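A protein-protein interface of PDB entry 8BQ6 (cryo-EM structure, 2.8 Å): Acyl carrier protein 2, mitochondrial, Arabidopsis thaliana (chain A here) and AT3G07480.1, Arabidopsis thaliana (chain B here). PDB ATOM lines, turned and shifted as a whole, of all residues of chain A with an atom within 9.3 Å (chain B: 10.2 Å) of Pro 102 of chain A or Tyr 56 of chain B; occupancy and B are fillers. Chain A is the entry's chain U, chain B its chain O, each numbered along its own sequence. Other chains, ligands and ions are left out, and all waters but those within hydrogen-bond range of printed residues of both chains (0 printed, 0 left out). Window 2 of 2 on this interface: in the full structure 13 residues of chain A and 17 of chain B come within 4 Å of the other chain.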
ATOM      1  N   VAL A  90     -25.543  11.771  29.929  1.00  0.00           N
ATOM      2  CA  VAL A  90     -25.337  11.192  28.564  1.00  0.00           C
ATOM      3  C   VAL A  90     -23.966  11.640  28.044  1.00  0.00           C
ATOM      4  O   VAL A  90     -23.266  10.790  27.474  1.00  0.00           O
ATOM      5  CB  VAL A  90     -26.474  11.576  27.602  1.00  0.00           C
ATOM      6  CG1 VAL A  90     -26.476  10.722  26.347  1.00  0.00           C
ATOM      7  CG2 VAL A  90     -27.832  11.529  28.284  1.00  0.00           C
ATOM      8  N   MET A  91     -23.590  12.909  28.254  1.00  0.00           N
ATOM      9  CA  MET A  91     -22.249  13.415  27.850  1.00  0.00           C
ATOM     10  C   MET A  91     -21.155  12.529  28.460  1.00  0.00           C
ATOM     11  O   MET A  91     -20.262  12.101  27.710  1.00  0.00           O
ATOM     12  CB  MET A  91     -22.033  14.851  28.339  1.00  0.00           C
ATOM     13  CG  MET A  91     -22.921  15.884  27.673  1.00  0.00           C
ATOM     14  SD  MET A  91     -23.114  15.618  25.898  1.00  0.00           S
ATOM     15  CE  MET A  91     -21.515  16.159  25.300  1.00  0.00           C
ATOM     16  N   GLU A  94     -20.971   9.178  26.642  1.00  0.00           N
ATOM     17  CA  GLU A  94     -20.332   9.398  25.316  1.00  0.00           C
ATOM     18  C   GLU A  94     -18.814   9.336  25.470  1.00  0.00           C
ATOM     19  O   GLU A  94     -18.199   8.514  24.784  1.00  0.00           O
ATOM     20  CB  GLU A  94     -20.679  10.784  24.785  1.00  0.00           C
ATOM     21  CG  GLU A  94     -22.022  10.873  24.098  1.00  0.00           C
ATOM     22  CD  GLU A  94     -22.611  12.269  24.024  1.00  0.00           C
ATOM     23  OE1 GLU A  94     -21.956  13.157  23.441  1.00  0.00           O
ATOM     24  OE2 GLU A  94     -23.729  12.463  24.544  1.00  0.00           O
ATOM     25  N   PHE A  99     -17.690   7.460  21.896  1.00  0.00           N
ATOM     26  CA  PHE A  99     -18.475   7.610  20.644  1.00  0.00           C
ATOM     27  C   PHE A  99     -19.543   8.690  20.851  1.00  0.00           C
ATOM     28  O   PHE A  99     -19.944   8.928  21.999  1.00  0.00           O
ATOM     29  CB  PHE A  99     -19.000   6.243  20.193  1.00  0.00           C
ATOM     30  CG  PHE A  99     -20.283   5.758  20.818  1.00  0.00           C
ATOM     31  CD1 PHE A  99     -20.298   5.223  22.095  1.00  0.00           C
ATOM     32  CD2 PHE A  99     -21.471   5.790  20.108  1.00  0.00           C
ATOM     33  CE1 PHE A  99     -21.475   4.763  22.660  1.00  0.00           C
ATOM     34  CE2 PHE A  99     -22.651   5.340  20.677  1.00  0.00           C
ATOM     35  CZ  PHE A  99     -22.650   4.815  21.948  1.00  0.00           C
ATOM     36  N   GLU A 100     -19.975   9.336  19.766  1.00  0.00           N
ATOM     37  CA  GLU A 100     -21.024  10.389  19.873  1.00  0.00           C
ATOM     38  C   GLU A 100     -22.410   9.736  19.916  1.00  0.00           C
ATOM     39  O   GLU A 100     -22.587   8.662  19.320  1.00  0.00           O
ATOM     40  CB  GLU A 100     -20.891  11.443  18.763  1.00  0.00           C
ATOM     41  CG  GLU A 100     -19.642  12.303  18.853  1.00  0.00           C
ATOM     42  CD  GLU A 100     -19.445  13.308  17.728  1.00  0.00           C
ATOM     43  OE1 GLU A 100     -20.196  13.231  16.735  1.00  0.00           O
ATOM     44  OE2 GLU A 100     -18.553  14.169  17.849  1.00  0.00           O
ATOM     45  N   ILE A 101     -23.353  10.367  20.620  1.00  0.00           N
ATOM     46  CA  ILE A 101     -24.743   9.833  20.724  1.00  0.00           C
ATOM     47  C   ILE A 101     -25.661  10.888  20.115  1.00  0.00           C
ATOM     48  O   ILE A 101     -25.617  12.043  20.580  1.00  0.00           O
ATOM     49  CB  ILE A 101     -25.109   9.491  22.182  1.00  0.00           C
ATOM     50  CG1 ILE A 101     -24.229   8.368  22.739  1.00  0.00           C
ATOM     51  CG2 ILE A 101     -26.588   9.162  22.320  1.00  0.00           C
ATOM     52  CD1 ILE A 101     -24.455   8.067  24.202  1.00  0.00           C
ATOM     53  N   PRO A 102     -26.492  10.595  19.066  1.00  0.00           N
ATOM     54  CA  PRO A 102     -27.313  11.630  18.432  1.00  0.00           C
ATOM     55  C   PRO A 102     -28.389  12.200  19.360  1.00  0.00           C
ATOM     56  O   PRO A 102     -28.778  11.505  20.255  1.00  0.00           O
ATOM     57  CB  PRO A 102     -28.113  10.905  17.349  1.00  0.00           C
ATOM     58  CG  PRO A 102     -27.307   9.681  17.037  1.00  0.00           C
ATOM     59  CD  PRO A 102     -26.738   9.291  18.379  1.00  0.00           C
ATOM     60  N   ASP A 103     -28.884  13.409  19.073  1.00  0.00           N
ATOM     61  CA  ASP A 103     -29.949  14.039  19.901  1.00  0.00           C
ATOM     62  C   ASP A 103     -31.165  13.112  19.973  1.00  0.00           C
ATOM     63  O   ASP A 103     -31.671  12.910  21.087  1.00  0.00           O
ATOM     64  CB  ASP A 103     -30.350  15.405  19.355  1.00  0.00           C
ATOM     65  CG  ASP A 103     -29.280  16.460  19.560  1.00  0.00           C
ATOM     66  OD1 ASP A 103     -28.359  16.214  20.367  1.00  0.00           O
ATOM     67  OD2 ASP A 103     -29.370  17.516  18.903  1.00  0.00           O
ATOM     68  N   ASN A 104     -31.610  12.575  18.838  1.00  0.00           N
ATOM     69  CA  ASN A 104     -32.732  11.598  18.820  1.00  0.00           C
ATOM     70  C   ASN A 104     -32.552  10.562  19.933  1.00  0.00           C
ATOM     71  O   ASN A 104     -33.527  10.320  20.661  1.00  0.00           O
ATOM     72  CB  ASN A 104     -32.829  10.880  17.473  1.00  0.00           C
ATOM     73  CG  ASN A 104     -33.320  11.767  16.349  1.00  0.00           C
ATOM     74  OD1 ASN A 104     -33.985  12.773  16.586  1.00  0.00           O
ATOM     75  ND2 ASN A 104     -32.996  11.402  15.120  1.00  0.00           N
ATOM     76  N   GLU A 105     -31.352   9.995  20.074  1.00  0.00           N
ATOM     77  CA  GLU A 105     -31.131   8.908  21.068  1.00  0.00           C
ATOM     78  C   GLU A 105     -30.613   9.467  22.392  1.00  0.00           C
ATOM     79  O   GLU A 105     -30.716   8.758  23.397  1.00  0.00           O
ATOM     80  CB  GLU A 105     -30.161   7.884  20.485  1.00  0.00           C
ATOM     81  CG  GLU A 105     -30.863   6.816  19.675  1.00  0.00           C
ATOM     82  CD  GLU A 105     -30.767   6.991  18.172  1.00  0.00           C
ATOM     83  OE1 GLU A 105     -31.797   7.319  17.553  1.00  0.00           O
ATOM     84  OE2 GLU A 105     -29.665   6.792  17.624  1.00  0.00           O
ATOM     85  N   ALA A 106     -30.059  10.684  22.388  1.00  0.00           N
ATOM     86  CA  ALA A 106     -29.610  11.315  23.651  1.00  0.00           C
ATOM     87  C   ALA A 106     -30.800  11.417  24.606  1.00  0.00           C
ATOM     88  O   ALA A 106     -30.589  11.204  25.812  1.00  0.00           O
ATOM     89  CB  ALA A 106     -29.004  12.666  23.381  1.00  0.00           C
ATOM     90  N   ASP A 107     -31.997  11.697  24.079  1.00  0.00           N
ATOM     91  CA  ASP A 107     -33.201  11.889  24.932  1.00  0.00           C
ATOM     92  C   ASP A 107     -33.742  10.538  25.413  1.00  0.00           C
ATOM     93  O   ASP A 107     -34.216  10.490  26.562  1.00  0.00           O
ATOM     94  CB  ASP A 107     -34.280  12.693  24.199  1.00  0.00           C
ATOM     95  CG  ASP A 107     -33.736  13.808  23.323  1.00  0.00           C
ATOM     96  OD1 ASP A 107     -32.774  14.479  23.752  1.00  0.00           O
ATOM     97  OD2 ASP A 107     -34.280  13.999  22.218  1.00  0.00           O
ATOM     98  N   LYS A 108     -33.680   9.499  24.573  1.00  0.00           N
ATOM     99  CA  LYS A 108     -34.224   8.162  24.935  1.00  0.00           C
ATOM    100  C   LYS A 108     -33.458   7.610  26.141  1.00  0.00           C
ATOM    101  O   LYS A 108     -34.012   6.759  26.853  1.00  0.00           O
ATOM    102  CB  LYS A 108     -34.176   7.237  23.712  1.00  0.00           C
ATOM    103  CG  LYS A 108     -35.091   7.595  22.547  1.00  0.00           C
ATOM    104  CD  LYS A 108     -34.984   6.660  21.359  1.00  0.00           C
ATOM    105  CE  LYS A 108     -35.914   7.011  20.215  1.00  0.00           C
ATOM    106  NZ  LYS A 108     -35.752   6.082  19.073  1.00  0.00           N
ATOM    107  N   ILE A 109     -32.233   8.094  26.366  1.00  0.00           N
ATOM    108  CA  ILE A 109     -31.441   7.661  27.548  1.00  0.00           C
ATOM    109  C   ILE A 109     -31.926   8.537  28.699  1.00  0.00           C
ATOM    110  O   ILE A 109     -31.353   9.628  28.924  1.00  0.00           O
ATOM    111  CB  ILE A 109     -29.933   7.773  27.250  1.00  0.00           C
ATOM    112  CG1 ILE A 109     -29.520   6.827  26.121  1.00  0.00           C
ATOM    113  CG2 ILE A 109     -29.092   7.556  28.498  1.00  0.00           C
ATOM    114  CD1 ILE A 109     -28.158   7.122  25.551  1.00  0.00           C
ATOM    115  N   PHE A 118     -28.497   0.644  24.612  1.00  0.00           N
ATOM    116  CA  PHE A 118     -27.989   1.418  23.448  1.00  0.00           C
ATOM    117  C   PHE A 118     -26.504   1.119  23.197  1.00  0.00           C
ATOM    118  O   PHE A 118     -26.177   0.742  22.069  1.00  0.00           O
ATOM    119  CB  PHE A 118     -28.252   2.904  23.665  1.00  0.00           C
ATOM    120  CG  PHE A 118     -27.837   3.801  22.529  1.00  0.00           C
ATOM    121  CD1 PHE A 118     -28.530   3.794  21.329  1.00  0.00           C
ATOM    122  CD2 PHE A 118     -26.757   4.659  22.659  1.00  0.00           C
ATOM    123  CE1 PHE A 118     -28.149   4.621  20.285  1.00  0.00           C
ATOM    124  CE2 PHE A 118     -26.377   5.483  21.614  1.00  0.00           C
ATOM    125  CZ  PHE A 118     -27.076   5.468  20.431  1.00  0.00           C
ATOM    126  N   HIS A 122     -24.517  -0.828  20.064  1.00  0.00           N
ATOM    127  CA  HIS A 122     -23.834   0.150  19.181  1.00  0.00           C
ATOM    128  C   HIS A 122     -22.420  -0.323  18.866  1.00  0.00           C
ATOM    129  O   HIS A 122     -21.651  -0.559  19.807  1.00  0.00           O
ATOM    130  CB  HIS A 122     -23.756   1.529  19.822  1.00  0.00           C
ATOM    131  CG  HIS A 122     -23.965   2.605  18.820  1.00  0.00           C
ATOM    132  ND1 HIS A 122     -22.960   3.036  17.984  1.00  0.00           N
ATOM    133  CD2 HIS A 122     -25.069   3.304  18.489  1.00  0.00           C
ATOM    134  CE1 HIS A 122     -23.430   3.975  17.195  1.00  0.00           C
ATOM    135  NE2 HIS A 122     -24.720   4.159  17.487  1.00  0.00           N
ATOM    136  N   PRO A 123     -22.021  -0.562  17.578  1.00  0.00           N
ATOM    137  CA  PRO A 123     -20.702  -1.154  17.277  1.00  0.00           C
ATOM    138  C   PRO A 123     -19.488  -0.223  17.416  1.00  0.00           C
ATOM    139  O   PRO A 123     -18.403  -0.728  17.571  1.00  0.00           O
ATOM    140  CB  PRO A 123     -20.818  -1.586  15.810  1.00  0.00           C
ATOM    141  CG  PRO A 123     -21.734  -0.575  15.199  1.00  0.00           C
ATOM    142  CD  PRO A 123     -22.741  -0.312  16.292  1.00  0.00           C
ATOM    143  N   GLN A 124     -19.701   1.090  17.356  1.00  0.00           N
ATOM    144  CA  GLN A 124     -18.609   2.084  17.489  1.00  0.00           C
ATOM    145  C   GLN A 124     -18.191   2.200  18.956  1.00  0.00           C
ATOM    146  O   GLN A 124     -17.116   2.772  19.208  1.00  0.00           O
ATOM    147  CB  GLN A 124     -19.102   3.425  16.958  1.00  0.00           C
ATOM    148  CG  GLN A 124     -19.563   3.362  15.511  1.00  0.00           C
ATOM    149  CD  GLN A 124     -20.002   4.707  14.989  1.00  0.00           C
ATOM    150  OE1 GLN A 124     -20.564   5.524  15.715  1.00  0.00           O
ATOM    151  NE2 GLN A 124     -19.753   4.942  13.713  1.00  0.00           N
ATOM    152  N   LEU B  48     -37.429  -4.279  13.343  1.00  0.00           N
ATOM    153  CA  LEU B  48     -35.991  -4.466  13.375  1.00  0.00           C
ATOM    154  C   LEU B  48     -35.306  -3.108  13.363  1.00  0.00           C
ATOM    155  O   LEU B  48     -35.867  -2.119  12.887  1.00  0.00           O
ATOM    156  CB  LEU B  48     -35.582  -5.312  12.176  1.00  0.00           C
ATOM    157  CG  LEU B  48     -34.149  -5.666  11.832  1.00  0.00           C
ATOM    158  CD1 LEU B  48     -33.673  -6.485  12.997  1.00  0.00           C
ATOM    159  CD2 LEU B  48     -34.076  -6.474  10.566  1.00  0.00           C
ATOM    160  N   SER B  49     -34.089  -3.065  13.897  1.00  0.00           N
ATOM    161  CA  SER B  49     -33.292  -1.848  13.901  1.00  0.00           C
ATOM    162  C   SER B  49     -31.912  -2.133  13.335  1.00  0.00           C
ATOM    163  O   SER B  49     -31.207  -3.021  13.814  1.00  0.00           O
ATOM    164  CB  SER B  49     -33.156  -1.266  15.308  1.00  0.00           C
ATOM    165  OG  SER B  49     -34.412  -0.842  15.802  1.00  0.00           O
ATOM    166  N   ALA B  50     -31.522  -1.362  12.333  1.00  0.00           N
ATOM    167  CA  ALA B  50     -30.214  -1.519  11.723  1.00  0.00           C
ATOM    168  C   ALA B  50     -29.400  -0.259  11.958  1.00  0.00           C
ATOM    169  O   ALA B  50     -29.928   0.854  11.892  1.00  0.00           O
ATOM    170  CB  ALA B  50     -30.327  -1.810  10.229  1.00  0.00           C
ATOM    171  N   ILE B  51     -28.117  -0.439  12.249  1.00  0.00           N
ATOM    172  CA  ILE B  51     -27.198   0.672  12.459  1.00  0.00           C
ATOM    173  C   ILE B  51     -26.263   0.736  11.263  1.00  0.00           C
ATOM    174  O   ILE B  51     -25.518  -0.214  10.993  1.00  0.00           O
ATOM    175  CB  ILE B  51     -26.413   0.518  13.767  1.00  0.00           C
ATOM    176  CG1 ILE B  51     -27.294   0.872  14.958  1.00  0.00           C
ATOM    177  CG2 ILE B  51     -25.208   1.430  13.767  1.00  0.00           C
ATOM    178  CD1 ILE B  51     -26.804   0.283  16.246  1.00  0.00           C
ATOM    179  N   ASP B  52     -26.296   1.856  10.553  1.00  0.00           N
ATOM    180  CA  ASP B  52     -25.507   2.006   9.348  1.00  0.00           C
ATOM    181  C   ASP B  52     -24.048   2.307   9.698  1.00  0.00           C
ATOM    182  O   ASP B  52     -23.722   2.585  10.854  1.00  0.00           O
ATOM    183  CB  ASP B  52     -26.114   3.099   8.472  1.00  0.00           C
ATOM    184  CG  ASP B  52     -26.210   4.420   9.177  1.00  0.00           C
ATOM    185  OD1 ASP B  52     -25.159   5.034   9.446  1.00  0.00           O
ATOM    186  OD2 ASP B  52     -27.347   4.852   9.443  1.00  0.00           O
ATOM    187  N   PRO B  53     -23.141   2.225   8.716  1.00  0.00           N
ATOM    188  CA  PRO B  53     -21.715   2.422   9.031  1.00  0.00           C
ATOM    189  C   PRO B  53     -21.403   3.771   9.654  1.00  0.00           C
ATOM    190  O   PRO B  53     -20.412   3.886  10.386  1.00  0.00           O
ATOM    191  CB  PRO B  53     -21.025   2.253   7.669  1.00  0.00           C
ATOM    192  CG  PRO B  53     -22.107   2.311   6.653  1.00  0.00           C
ATOM    193  CD  PRO B  53     -23.341   1.837   7.310  1.00  0.00           C
ATOM    194  N   ASP B  54     -22.213   4.798   9.395  1.00  0.00           N
ATOM    195  CA  ASP B  54     -22.022   6.071  10.078  1.00  0.00           C
ATOM    196  C   ASP B  54     -22.654   6.107  11.463  1.00  0.00           C
ATOM    197  O   ASP B  54     -22.771   7.193  12.039  1.00  0.00           O
ATOM    198  CB  ASP B  54     -22.574   7.212   9.229  1.00  0.00           C
ATOM    199  CG  ASP B  54     -21.730   7.478   8.010  1.00  0.00           C
ATOM    200  OD1 ASP B  54     -20.584   6.984   7.969  1.00  0.00           O
ATOM    201  OD2 ASP B  54     -22.206   8.185   7.097  1.00  0.00           O
ATOM    202  N   GLY B  55     -23.066   4.964  12.004  1.00  0.00           N
ATOM    203  CA  GLY B  55     -23.486   4.869  13.384  1.00  0.00           C
ATOM    204  C   GLY B  55     -24.909   5.295  13.673  1.00  0.00           C
ATOM    205  O   GLY B  55     -25.291   5.345  14.846  1.00  0.00           O
ATOM    206  N   TYR B  56     -25.687   5.577  12.627  1.00  0.00           N
ATOM    207  CA  TYR B  56     -27.073   6.076  12.828  1.00  0.00           C
ATOM    208  C   TYR B  56     -28.071   4.922  12.852  1.00  0.00           C
ATOM    209  O   TYR B  56     -28.018   4.046  11.988  1.00  0.00           O
ATOM    210  CB  TYR B  56     -27.390   7.157  11.795  1.00  0.00           C
ATOM    211  CG  TYR B  56     -26.612   8.415  12.075  1.00  0.00           C
ATOM    212  CD1 TYR B  56     -26.771   9.080  13.279  1.00  0.00           C
ATOM    213  CD2 TYR B  56     -25.675   8.902  11.181  1.00  0.00           C
ATOM    214  CE1 TYR B  56     -26.046  10.221  13.575  1.00  0.00           C
ATOM    215  CE2 TYR B  56     -24.942  10.043  11.461  1.00  0.00           C
ATOM    216  CZ  TYR B  56     -25.129  10.705  12.662  1.00  0.00           C
ATOM    217  OH  TYR B  56     -24.421  11.835  12.950  1.00  0.00           O
ATOM    218  N   LYS B  57     -28.968   4.934  13.829  1.00  0.00           N
ATOM    219  CA  LYS B  57     -29.945   3.874  13.993  1.00  0.00           C
ATOM    220  C   LYS B  57     -31.204   4.153  13.182  1.00  0.00           C
ATOM    221  O   LYS B  57     -31.710   5.278  13.159  1.00  0.00           O
ATOM    222  CB  LYS B  57     -30.304   3.713  15.467  1.00  0.00           C
ATOM    223  CG  LYS B  57     -31.033   2.435  15.755  1.00  0.00           C
ATOM    224  CD  LYS B  57     -31.889   2.568  16.986  1.00  0.00           C
ATOM    225  CE  LYS B  57     -31.068   2.950  18.198  1.00  0.00           C
ATOM    226  NZ  LYS B  57     -31.333   1.978  19.289  1.00  0.00           N
ATOM    227  N   GLN B  58     -31.711   3.114  12.524  1.00  0.00           N
ATOM    228  CA  GLN B  58     -32.908   3.208  11.703  1.00  0.00           C
ATOM    229  C   GLN B  58     -33.816   2.023  11.977  1.00  0.00           C
ATOM    230  O   GLN B  58     -33.341   0.914  12.231  1.00  0.00           O
ATOM    231  CB  GLN B  58     -32.560   3.231  10.227  1.00  0.00           C
ATOM    232  CG  GLN B  58     -31.996   4.531   9.761  1.00  0.00           C
ATOM    233  CD  GLN B  58     -30.884   4.312   8.782  1.00  0.00           C
ATOM    234  OE1 GLN B  58     -30.687   3.200   8.299  1.00  0.00           O
ATOM    235  NE2 GLN B  58     -30.135   5.363   8.490  1.00  0.00           N
ATOM    236  N   ASP B  59     -35.122   2.253  11.894  1.00  0.00           N
ATOM    237  CA  ASP B  59     -36.107   1.204  12.121  1.00  0.00           C
ATOM    238  C   ASP B  59     -36.555   0.619  10.788  1.00  0.00           C
ATOM    239  O   ASP B  59     -37.240   1.293  10.012  1.00  0.00           O
ATOM    240  CB  ASP B  59     -37.305   1.754  12.888  1.00  0.00           C
ATOM    241  CG  ASP B  59     -37.067   1.796  14.377  1.00  0.00           C
ATOM    242  OD1 ASP B  59     -35.931   1.518  14.808  1.00  0.00           O
ATOM    243  OD2 ASP B  59     -38.025   2.086  15.120  1.00  0.00           O
ATOM    244  N   ILE B  60     -36.188  -0.633  10.526  1.00  0.00           N
ATOM    245  CA  ILE B  60     -36.490  -1.269   9.253  1.00  0.00           C
ATOM    246  C   ILE B  60     -37.557  -2.338   9.462  1.00  0.00           C
ATOM    247  O   ILE B  60     -37.870  -2.735  10.584  1.00  0.00           O
ATOM    248  CB  ILE B  60     -35.245  -1.870   8.580  1.00  0.00           C
ATOM    249  CG1 ILE B  60     -34.881  -3.200   9.229  1.00  0.00           C
ATOM    250  CG2 ILE B  60     -34.083  -0.893   8.640  1.00  0.00           C
ATOM    251  CD1 ILE B  60     -33.609  -3.778   8.708  1.00  0.00           C
ATOM    252  N   LEU B  72     -33.202  -5.712   4.560  1.00  0.00           N
ATOM    253  CA  LEU B  72     -32.189  -4.670   4.468  1.00  0.00           C
ATOM    254  C   LEU B  72     -32.215  -3.970   3.115  1.00  0.00           C
ATOM    255  O   LEU B  72     -31.972  -2.761   3.043  1.00  0.00           O
ATOM    256  CB  LEU B  72     -30.817  -5.268   4.747  1.00  0.00           C
ATOM    257  CG  LEU B  72     -30.577  -5.509   6.235  1.00  0.00           C
ATOM    258  CD1 LEU B  72     -29.358  -6.366   6.433  1.00  0.00           C
ATOM    259  CD2 LEU B  72     -30.417  -4.185   6.946  1.00  0.00           C
ATOM    260  N   LEU B  77     -30.364  -0.095   2.437  1.00  0.00           N
ATOM    261  CA  LEU B  77     -29.244  -0.215   3.363  1.00  0.00           C
ATOM    262  C   LEU B  77     -28.159  -1.107   2.789  1.00  0.00           C
ATOM    263  O   LEU B  77     -26.966  -0.885   3.020  1.00  0.00           O
ATOM    264  CB  LEU B  77     -29.734  -0.763   4.697  1.00  0.00           C
ATOM    265  CG  LEU B  77     -30.467   0.269   5.541  1.00  0.00           C
ATOM    266  CD1 LEU B  77     -30.960  -0.374   6.811  1.00  0.00           C
ATOM    267  CD2 LEU B  77     -29.550   1.445   5.846  1.00  0.00           C
ATOM    268  N   VAL B 147     -31.404  -6.023  16.764  1.00  0.00           N
ATOM    269  CA  VAL B 147     -30.612  -4.892  16.295  1.00  0.00           C
ATOM    270  C   VAL B 147     -29.436  -5.426  15.498  1.00  0.00           C
ATOM    271  O   VAL B 147     -28.774  -6.384  15.916  1.00  0.00           O
ATOM    272  CB  VAL B 147     -30.136  -4.006  17.456  1.00  0.00           C
ATOM    273  CG1 VAL B 147     -29.290  -2.858  16.927  1.00  0.00           C
ATOM    274  CG2 VAL B 147     -31.323  -3.463  18.212  1.00  0.00           C
ATOM    275  N   VAL B 148     -29.177  -4.808  14.352  1.00  0.00           N
ATOM    276  CA  VAL B 148     -28.192  -5.285  13.398  1.00  0.00           C
ATOM    277  C   VAL B 148     -27.289  -4.118  13.023  1.00  0.00           C
ATOM    278  O   VAL B 148     -27.745  -2.973  12.936  1.00  0.00           O
ATOM    279  CB  VAL B 148     -28.888  -5.888  12.160  1.00  0.00           C
ATOM    280  CG1 VAL B 148     -27.974  -5.900  10.962  1.00  0.00           C
ATOM    281  CG2 VAL B 148     -29.400  -7.281  12.476  1.00  0.00           C
ATOM    282  N   ALA B 149     -26.003  -4.398  12.847  1.00  0.00           N
ATOM    283  CA  ALA B 149     -25.043  -3.405  12.387  1.00  0.00           C
ATOM    284  C   ALA B 149     -24.621  -3.735  10.962  1.00  0.00           C
ATOM    285  O   ALA B 149     -24.244  -4.874  10.669  1.00  0.00           O
ATOM    286  CB  ALA B 149     -23.824  -3.357  13.308  1.00  0.00           C
ATOM    287  N   VAL B 150     -24.681  -2.739  10.086  1.00  0.00           N
ATOM    288  CA  VAL B 150     -24.352  -2.903   8.673  1.00  0.00           C
ATOM    289  C   VAL B 150     -22.982  -2.269   8.440  1.00  0.00           C
ATOM    290  O   VAL B 150     -22.852  -1.042   8.571  1.00  0.00           O
ATOM    291  CB  VAL B 150     -25.418  -2.266   7.774  1.00  0.00           C
ATOM    292  CG1 VAL B 150     -24.994  -2.327   6.323  1.00  0.00           C
ATOM    293  CG2 VAL B 150     -26.753  -2.956   7.976  1.00  0.00           C
ATOM    294  N   PRO B 151     -21.954  -3.041   8.113  1.00  0.00           N
ATOM    295  CA  PRO B 151     -20.632  -2.454   7.877  1.00  0.00           C
ATOM    296  C   PRO B 151     -20.564  -1.764   6.520  1.00  0.00           C
ATOM    297  O   PRO B 151     -21.519  -1.751   5.743  1.00  0.00           O
ATOM    298  CB  PRO B 151     -19.693  -3.660   7.939  1.00  0.00           C
ATOM    299  CG  PRO B 151     -20.541  -4.815   7.550  1.00  0.00           C
ATOM    300  CD  PRO B 151     -21.944  -4.509   7.989  1.00  0.00           C
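O of Gly 55 of chain B is in hydrogen-bond range of NE2 of His 122 of chain A (3.0 Å).
The backbone NH of Ile 51 of chain B lies within hydrogen-bond range of the backbone carbonyl oxygen of Val 148 of chain B (2.7 Å). The side-chain carboxylate of Asp 52 of chain B is in hydrogen-bond range of the backbone NH of Gly 55 of chain B (3.3 Å). O of Ile 51 of chain B sits at hydrogen-bond distance from N of Val 150 of chain B, 2.8 Å away. The side-chain carboxylate (OD1) of Asp 52 of chain B is in hydrogen-bond range of the backbone NH (N) of Asp 54 of chain B (3.0 Å). The side-chain carboxylate (OD1) of Asp 52 of chain B is in hydrogen-bond range of the backbone NH (N) of Tyr 56 of chain B, at 3.3 Å.
Tyr 56 of chain B touches Pro 102 of chain A. Lys 57 of chain B touches Glu 105 of chain A (CB to OE2, 3.8 Å). Phe 118 of chain A touches Lys 57 of chain B. Pro 123 of chain A touches Ile 51 of chain B. Ala 149 of chain B touches Pro 123 of chain A. Pro 53 of chain B touches Gln 124 of chain A (O to NE2, 3.6 Å). Asp 54 of chain B touches Gln 124 of chain A. Gly 55 of chain B touches Gln 124 of chain A.
Pro 102 of chain A touches just one residue of chain B: Tyr 56 (3.7 Å). Of chain A, only Pro 102 (3.7 Å) comes within 4 Å of Tyr 56 of chain B. No residue of chain B comes within 4 Å of Asp 103 of chain A. No residue of chain B comes within 4 Å of Ala 106 of chain A. No residue of chain A comes within 4 Å of Asp 52 of chain B. Gly 55 of chain B touches two residues of chain A. Of the printed residues of chain A, Ile 51 of chain B touches Pro 123. Of the printed residues of chain A, Pro 53 of chain B touches Gln 124 (3.6 Å). Val 90 of chain A touches none of the printed residues of chain B.
Of the 20 printed residues of chain B, 7 touch a printed residue of chain A. Hydrophobic or aromatic side chains of chain B that line the printed part of chain A: Ile 51, Tyr 56 and Ala 149. Hydrophobic or aromatic side chains of chain A within 4 Å of the printed part of chain B: Pro 102, Phe 118, His 122 and Pro 123. Along chain A the printed residues that touch a printed residue of chain B span positions 102 to 124. Among the printed residues, no Asp or Glu carboxylate lies within 4 Å of a Lys or Arg side-chain nitrogen of the other chain.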
